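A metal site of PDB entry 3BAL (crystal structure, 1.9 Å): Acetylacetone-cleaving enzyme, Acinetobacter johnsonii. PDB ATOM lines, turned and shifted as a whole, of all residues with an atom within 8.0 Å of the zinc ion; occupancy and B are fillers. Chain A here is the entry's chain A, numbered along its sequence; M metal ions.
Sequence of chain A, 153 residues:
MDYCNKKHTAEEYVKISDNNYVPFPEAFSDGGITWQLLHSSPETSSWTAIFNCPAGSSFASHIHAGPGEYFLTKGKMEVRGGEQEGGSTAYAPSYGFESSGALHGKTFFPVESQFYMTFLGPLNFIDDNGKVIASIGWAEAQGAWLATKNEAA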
ATOM      1  N   PHE A  59     -17.164  -6.929 -16.935  1.00  0.00           N
ATOM      2  CA  PHE A  59     -15.957  -7.013 -16.108  1.00  0.00           C
ATOM      3  C   PHE A  59     -15.241  -8.323 -16.407  1.00  0.00           C
ATOM      4  O   PHE A  59     -15.873  -9.310 -16.772  1.00  0.00           O
ATOM      5  CB  PHE A  59     -16.304  -6.964 -14.618  1.00  0.00           C
ATOM      6  CG  PHE A  59     -16.765  -5.616 -14.125  1.00  0.00           C
ATOM      7  CD1 PHE A  59     -18.131  -5.311 -14.032  1.00  0.00           C
ATOM      8  CD2 PHE A  59     -15.834  -4.665 -13.722  1.00  0.00           C
ATOM      9  CE1 PHE A  59     -18.551  -4.073 -13.533  1.00  0.00           C
ATOM     10  CE2 PHE A  59     -16.243  -3.421 -13.231  1.00  0.00           C
ATOM     11  CZ  PHE A  59     -17.607  -3.128 -13.132  1.00  0.00           C
ATOM     12  N   ALA A  60     -13.918  -8.328 -16.251  1.00  0.00           N
ATOM     13  CA  ALA A  60     -13.110  -9.524 -16.481  1.00  0.00           C
ATOM     14  C   ALA A  60     -13.475 -10.558 -15.413  1.00  0.00           C
ATOM     15  O   ALA A  60     -14.004 -10.202 -14.363  1.00  0.00           O
ATOM     16  CB  ALA A  60     -11.632  -9.184 -16.402  1.00  0.00           C
ATOM     17  N   SER A  61     -13.181 -11.824 -15.696  1.00  0.00           N
ATOM     18  CA  SER A  61     -13.486 -12.929 -14.788  1.00  0.00           C
ATOM     19  C   SER A  61     -12.833 -12.813 -13.411  1.00  0.00           C
ATOM     20  O   SER A  61     -11.636 -12.566 -13.296  1.00  0.00           O
ATOM     21  CB  SER A  61     -13.074 -14.270 -15.418  1.00  0.00           C
ATOM     22  OG  SER A  61     -13.794 -14.511 -16.603  1.00  0.00           O
ATOM     23  N   HIS A  62     -13.629 -13.017 -12.365  1.00  0.00           N
ATOM     24  CA  HIS A  62     -13.101 -12.919 -11.014  1.00  0.00           C
ATOM     25  C   HIS A  62     -13.918 -13.696  -9.993  1.00  0.00           C
ATOM     26  O   HIS A  62     -15.057 -14.090 -10.241  1.00  0.00           O
ATOM     27  CB  HIS A  62     -13.050 -11.460 -10.574  1.00  0.00           C
ATOM     28  CG  HIS A  62     -14.390 -10.781 -10.605  1.00  0.00           C
ATOM     29  ND1 HIS A  62     -14.940 -10.268 -11.760  1.00  0.00           N
ATOM     30  CD2 HIS A  62     -15.295 -10.566  -9.627  1.00  0.00           C
ATOM     31  CE1 HIS A  62     -16.125  -9.766 -11.495  1.00  0.00           C
ATOM     32  NE2 HIS A  62     -16.371  -9.932 -10.209  1.00  0.00           N
ATOM     33  N   ILE A  63     -13.310 -13.891  -8.831  1.00  0.00           N
ATOM     34  CA  ILE A  63     -13.933 -14.593  -7.721  1.00  0.00           C
ATOM     35  C   ILE A  63     -13.956 -13.645  -6.518  1.00  0.00           C
ATOM     36  O   ILE A  63     -12.973 -12.949  -6.250  1.00  0.00           O
ATOM     37  CB  ILE A  63     -13.124 -15.853  -7.346  1.00  0.00           C
ATOM     38  CG1 ILE A  63     -13.125 -16.843  -8.511  1.00  0.00           C
ATOM     39  CG2 ILE A  63     -13.686 -16.478  -6.085  1.00  0.00           C
ATOM     40  CD1 ILE A  63     -12.255 -18.062  -8.300  1.00  0.00           C
ATOM     41  N   HIS A  64     -15.081 -13.611  -5.808  1.00  0.00           N
ATOM     42  CA  HIS A  64     -15.222 -12.783  -4.614  1.00  0.00           C
ATOM     43  C   HIS A  64     -14.685 -13.557  -3.419  1.00  0.00           C
ATOM     44  O   HIS A  64     -15.199 -14.615  -3.060  1.00  0.00           O
ATOM     45  CB  HIS A  64     -16.698 -12.439  -4.370  1.00  0.00           C
ATOM     46  CG  HIS A  64     -17.230 -11.399  -5.309  1.00  0.00           C
ATOM     47  ND1 HIS A  64     -17.434 -10.083  -4.922  1.00  0.00           N
ATOM     48  CD2 HIS A  64     -17.514 -11.450  -6.627  1.00  0.00           C
ATOM     49  CE1 HIS A  64     -17.823  -9.377  -5.967  1.00  0.00           C
ATOM     50  NE2 HIS A  64     -17.878 -10.190  -7.020  1.00  0.00           N
ATOM     51  N   GLY A  68     -20.133  -9.461  -0.858  1.00  0.00           N
ATOM     52  CA  GLY A  68     -20.272  -8.169  -1.516  1.00  0.00           C
ATOM     53  C   GLY A  68     -21.752  -7.886  -1.680  1.00  0.00           C
ATOM     54  O   GLY A  68     -22.537  -8.814  -1.931  1.00  0.00           O
ATOM     55  N   TYR A  70     -24.655  -5.238  -3.616  1.00  0.00           N
ATOM     56  CA  TYR A  70     -24.875  -4.188  -4.590  1.00  0.00           C
ATOM     57  C   TYR A  70     -26.288  -3.586  -4.641  1.00  0.00           C
ATOM     58  O   TYR A  70     -27.283  -4.262  -4.358  1.00  0.00           O
ATOM     59  CB  TYR A  70     -24.471  -4.687  -5.998  1.00  0.00           C
ATOM     60  CG  TYR A  70     -25.393  -5.752  -6.590  1.00  0.00           C
ATOM     61  CD1 TYR A  70     -26.634  -5.414  -7.121  1.00  0.00           C
ATOM     62  CD2 TYR A  70     -25.015  -7.093  -6.587  1.00  0.00           C
ATOM     63  CE1 TYR A  70     -27.499  -6.392  -7.632  1.00  0.00           C
ATOM     64  CE2 TYR A  70     -25.867  -8.077  -7.100  1.00  0.00           C
ATOM     65  CZ  TYR A  70     -27.105  -7.718  -7.624  1.00  0.00           C
ATOM     66  OH  TYR A  70     -27.960  -8.688  -8.094  1.00  0.00           O
ATOM     67  N   MET A  77     -28.389  -5.693 -14.926  1.00  0.00           N
ATOM     68  CA  MET A  77     -27.105  -6.381 -14.752  1.00  0.00           C
ATOM     69  C   MET A  77     -27.251  -7.917 -14.711  1.00  0.00           C
ATOM     70  O   MET A  77     -28.017  -8.438 -13.891  1.00  0.00           O
ATOM     71  CB  MET A  77     -26.429  -5.878 -13.469  1.00  0.00           C
ATOM     72  CG  MET A  77     -25.118  -6.583 -13.106  1.00  0.00           C
ATOM     73  SD  MET A  77     -24.317  -5.823 -11.684  1.00  0.00           S
ATOM     74  CE  MET A  77     -25.402  -6.375 -10.372  1.00  0.00           C
ATOM     75  N   VAL A  79     -25.751 -11.235 -13.649  1.00  0.00           N
ATOM     76  CA  VAL A  79     -24.758 -11.812 -12.740  1.00  0.00           C
ATOM     77  C   VAL A  79     -24.810 -13.331 -12.768  1.00  0.00           C
ATOM     78  O   VAL A  79     -25.892 -13.933 -12.785  1.00  0.00           O
ATOM     79  CB  VAL A  79     -25.001 -11.358 -11.284  1.00  0.00           C
ATOM     80  CG1 VAL A  79     -23.780 -11.671 -10.436  1.00  0.00           C
ATOM     81  CG2 VAL A  79     -25.334  -9.881 -11.233  1.00  0.00           C
ATOM     82  N   ARG A  80     -23.645 -13.956 -12.748  1.00  0.00           N
ATOM     83  CA  ARG A  80     -23.542 -15.406 -12.774  1.00  0.00           C
ATOM     84  C   ARG A  80     -24.240 -16.007 -13.985  1.00  0.00           C
ATOM     85  O   ARG A  80     -24.885 -17.056 -13.893  1.00  0.00           O
ATOM     86  CB  ARG A  80     -24.100 -15.987 -11.477  1.00  0.00           C
ATOM     87  CG  ARG A  80     -23.175 -15.769 -10.284  1.00  0.00           C
ATOM     88  CD  ARG A  80     -23.786 -16.177  -8.961  1.00  0.00           C
ATOM     89  NE  ARG A  80     -24.729 -15.191  -8.440  1.00  0.00           N
ATOM     90  CZ  ARG A  80     -26.047 -15.266  -8.562  1.00  0.00           C
ATOM     91  NH1 ARG A  80     -26.600 -16.304  -9.182  1.00  0.00           N
ATOM     92  NH2 ARG A  80     -26.816 -14.302  -8.079  1.00  0.00           N
ATOM     93  N   GLU A  98     -23.885 -11.165  -3.015  1.00  0.00           N
ATOM     94  CA  GLU A  98     -23.013 -12.122  -3.684  1.00  0.00           C
ATOM     95  C   GLU A  98     -22.010 -12.564  -2.631  1.00  0.00           C
ATOM     96  O   GLU A  98     -21.157 -11.795  -2.187  1.00  0.00           O
ATOM     97  CB  GLU A  98     -22.324 -11.456  -4.875  1.00  0.00           C
ATOM     98  CG  GLU A  98     -23.278 -11.008  -5.999  1.00  0.00           C
ATOM     99  CD  GLU A  98     -23.927 -12.171  -6.737  1.00  0.00           C
ATOM    100  OE1 GLU A  98     -23.223 -13.161  -7.027  1.00  0.00           O
ATOM    101  OE2 GLU A  98     -25.143 -12.103  -7.035  1.00  0.00           O
ATOM    102  N   ALA A 102     -18.272 -16.559  -4.772  1.00  0.00           N
ATOM    103  CA  ALA A 102     -19.031 -16.301  -5.984  1.00  0.00           C
ATOM    104  C   ALA A 102     -18.118 -16.118  -7.195  1.00  0.00           C
ATOM    105  O   ALA A 102     -17.220 -15.279  -7.177  1.00  0.00           O
ATOM    106  CB  ALA A 102     -19.931 -15.084  -5.798  1.00  0.00           C
ATOM    107  N   LEU A 103     -18.371 -16.899  -8.242  1.00  0.00           N
ATOM    108  CA  LEU A 103     -17.586 -16.820  -9.475  1.00  0.00           C
ATOM    109  C   LEU A 103     -18.316 -16.011 -10.535  1.00  0.00           C
ATOM    110  O   LEU A 103     -19.383 -16.406 -10.999  1.00  0.00           O
ATOM    111  CB  LEU A 103     -17.332 -18.234 -10.006  1.00  0.00           C
ATOM    112  CG  LEU A 103     -16.553 -18.335 -11.313  1.00  0.00           C
ATOM    113  CD1 LEU A 103     -15.137 -17.780 -11.143  1.00  0.00           C
ATOM    114  CD2 LEU A 103     -16.483 -19.797 -11.735  1.00  0.00           C
ATOM    115  N   HIS A 104     -17.729 -14.878 -10.924  1.00  0.00           N
ATOM    116  CA  HIS A 104     -18.326 -14.011 -11.929  1.00  0.00           C
ATOM    117  C   HIS A 104     -17.494 -13.968 -13.205  1.00  0.00           C
ATOM    118  O   HIS A 104     -16.601 -13.123 -13.356  1.00  0.00           O
ATOM    119  CB  HIS A 104     -18.491 -12.606 -11.361  1.00  0.00           C
ATOM    120  CG  HIS A 104     -19.439 -12.528 -10.195  1.00  0.00           C
ATOM    121  ND1 HIS A 104     -19.464 -11.471  -9.325  1.00  0.00           N
ATOM    122  CD2 HIS A 104     -20.407 -13.380  -9.777  1.00  0.00           C
ATOM    123  CE1 HIS A 104     -20.403 -11.666  -8.417  1.00  0.00           C
ATOM    124  NE2 HIS A 104     -20.988 -12.828  -8.671  1.00  0.00           N
ATOM    125  N   GLY A 105     -17.794 -14.899 -14.113  1.00  0.00           N
ATOM    126  CA  GLY A 105     -17.077 -15.011 -15.370  1.00  0.00           C
ATOM    127  C   GLY A 105     -17.096 -13.765 -16.245  1.00  0.00           C
ATOM    128  O   GLY A 105     -16.055 -13.334 -16.733  1.00  0.00           O
ATOM    129  N   THR A 107     -19.677 -10.532 -15.727  1.00  0.00           N
ATOM    130  CA  THR A 107     -20.826  -9.728 -15.324  1.00  0.00           C
ATOM    131  C   THR A 107     -21.075  -8.773 -16.496  1.00  0.00           C
ATOM    132  O   THR A 107     -20.177  -8.007 -16.879  1.00  0.00           O
ATOM    133  CB  THR A 107     -20.536  -8.953 -14.011  1.00  0.00           C
ATOM    134  OG1 THR A 107     -20.357  -9.890 -12.944  1.00  0.00           O
ATOM    135  CG2 THR A 107     -21.688  -8.028 -13.669  1.00  0.00           C
ATOM    136  N   PHE A 115     -24.453   1.147 -10.642  1.00  0.00           N
ATOM    137  CA  PHE A 115     -24.603   0.382  -9.418  1.00  0.00           C
ATOM    138  C   PHE A 115     -23.556   0.757  -8.367  1.00  0.00           C
ATOM    139  O   PHE A 115     -22.407   1.086  -8.694  1.00  0.00           O
ATOM    140  CB  PHE A 115     -24.584  -1.139  -9.713  1.00  0.00           C
ATOM    141  CG  PHE A 115     -23.207  -1.704  -9.977  1.00  0.00           C
ATOM    142  CD1 PHE A 115     -22.469  -2.283  -8.948  1.00  0.00           C
ATOM    143  CD2 PHE A 115     -22.677  -1.690 -11.255  1.00  0.00           C
ATOM    144  CE1 PHE A 115     -21.213  -2.842  -9.196  1.00  0.00           C
ATOM    145  CE2 PHE A 115     -21.419  -2.239 -11.517  1.00  0.00           C
ATOM    146  CZ  PHE A 115     -20.685  -2.828 -10.488  1.00  0.00           C
ATOM    147  N   MET A 117     -21.682  -0.521  -4.775  1.00  0.00           N
ATOM    148  CA  MET A 117     -21.363  -1.793  -4.155  1.00  0.00           C
ATOM    149  C   MET A 117     -20.284  -1.713  -3.072  1.00  0.00           C
ATOM    150  O   MET A 117     -19.335  -0.927  -3.175  1.00  0.00           O
ATOM    151  CB  MET A 117     -20.937  -2.781  -5.249  1.00  0.00           C
ATOM    152  CG  MET A 117     -20.669  -4.215  -4.805  1.00  0.00           C
ATOM    153  SD  MET A 117     -20.717  -5.384  -6.224  1.00  0.00           S
ATOM    154  CE  MET A 117     -20.694  -7.002  -5.394  1.00  0.00           C
ATOM    155  N   PHE A 119     -17.561  -4.097  -0.763  1.00  0.00           N
ATOM    156  CA  PHE A 119     -16.848  -5.373  -0.825  1.00  0.00           C
ATOM    157  C   PHE A 119     -16.063  -5.650   0.462  1.00  0.00           C
ATOM    158  O   PHE A 119     -15.462  -4.739   1.036  1.00  0.00           O
ATOM    159  CB  PHE A 119     -15.815  -5.413  -1.972  1.00  0.00           C
ATOM    160  CG  PHE A 119     -16.325  -4.928  -3.305  1.00  0.00           C
ATOM    161  CD1 PHE A 119     -16.323  -3.567  -3.616  1.00  0.00           C
ATOM    162  CD2 PHE A 119     -16.776  -5.820  -4.278  1.00  0.00           C
ATOM    163  CE1 PHE A 119     -16.758  -3.103  -4.853  1.00  0.00           C
ATOM    164  CE2 PHE A 119     -17.214  -5.377  -5.522  1.00  0.00           C
ATOM    165  CZ  PHE A 119     -17.206  -4.008  -5.819  1.00  0.00           C
ATOM    166  N   LEU A 123     -11.047  -9.069  -4.802  1.00  0.00           N
ATOM    167  CA  LEU A 123     -11.673  -9.703  -5.952  1.00  0.00           C
ATOM    168  C   LEU A 123     -10.503 -10.320  -6.689  1.00  0.00           C
ATOM    169  O   LEU A 123      -9.591  -9.608  -7.117  1.00  0.00           O
ATOM    170  CB  LEU A 123     -12.352  -8.666  -6.850  1.00  0.00           C
ATOM    171  CG  LEU A 123     -13.470  -7.835  -6.222  1.00  0.00           C
ATOM    172  CD1 LEU A 123     -14.226  -7.139  -7.345  1.00  0.00           C
ATOM    173  CD2 LEU A 123     -14.418  -8.713  -5.414  1.00  0.00           C
ATOM    174  N   PHE A 125      -8.998 -11.825  -9.804  1.00  0.00           N
ATOM    175  CA  PHE A 125      -9.199 -11.978 -11.244  1.00  0.00           C
ATOM    176  C   PHE A 125      -8.378 -13.180 -11.690  1.00  0.00           C
ATOM    177  O   PHE A 125      -7.223 -13.314 -11.307  1.00  0.00           O
ATOM    178  CB  PHE A 125      -8.805 -10.698 -11.982  1.00  0.00           C
ATOM    179  CG  PHE A 125      -9.755  -9.553 -11.726  1.00  0.00           C
ATOM    180  CD1 PHE A 125      -9.630  -8.770 -10.576  1.00  0.00           C
ATOM    181  CD2 PHE A 125     -10.821  -9.306 -12.597  1.00  0.00           C
ATOM    182  CE1 PHE A 125     -10.545  -7.753 -10.300  1.00  0.00           C
ATOM    183  CE2 PHE A 125     -11.739  -8.289 -12.335  1.00  0.00           C
ATOM    184  CZ  PHE A 125     -11.606  -7.509 -11.178  1.00  0.00           C
HETATM  185 ZN    ZN M   1     -18.261  -9.798  -9.015  1.00  0.00          ZN
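The backbone carbonyl oxygen (O) of Ala 102 sits at hydrogen-bond distance from the backbone NH (N) of His 64, at 3.0 Å.
A ring nitrogen (NE2) of His 104 sits at hydrogen-bond distance from the side-chain carboxylate (OE1) of Glu 98, 2.8 Å away.
ND1 of His 62 is in hydrogen-bond range of O of Ala 60, at 2.8 Å.
The zinc ion is bound by NE2 of His 64.
A ring nitrogen (ND1) of His 104 binds the zinc ion (2.1 Å).
NE2 of His 62 is bound to the zinc ion (2.2 Å).
The zinc ion has three donor atoms within binding distance.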
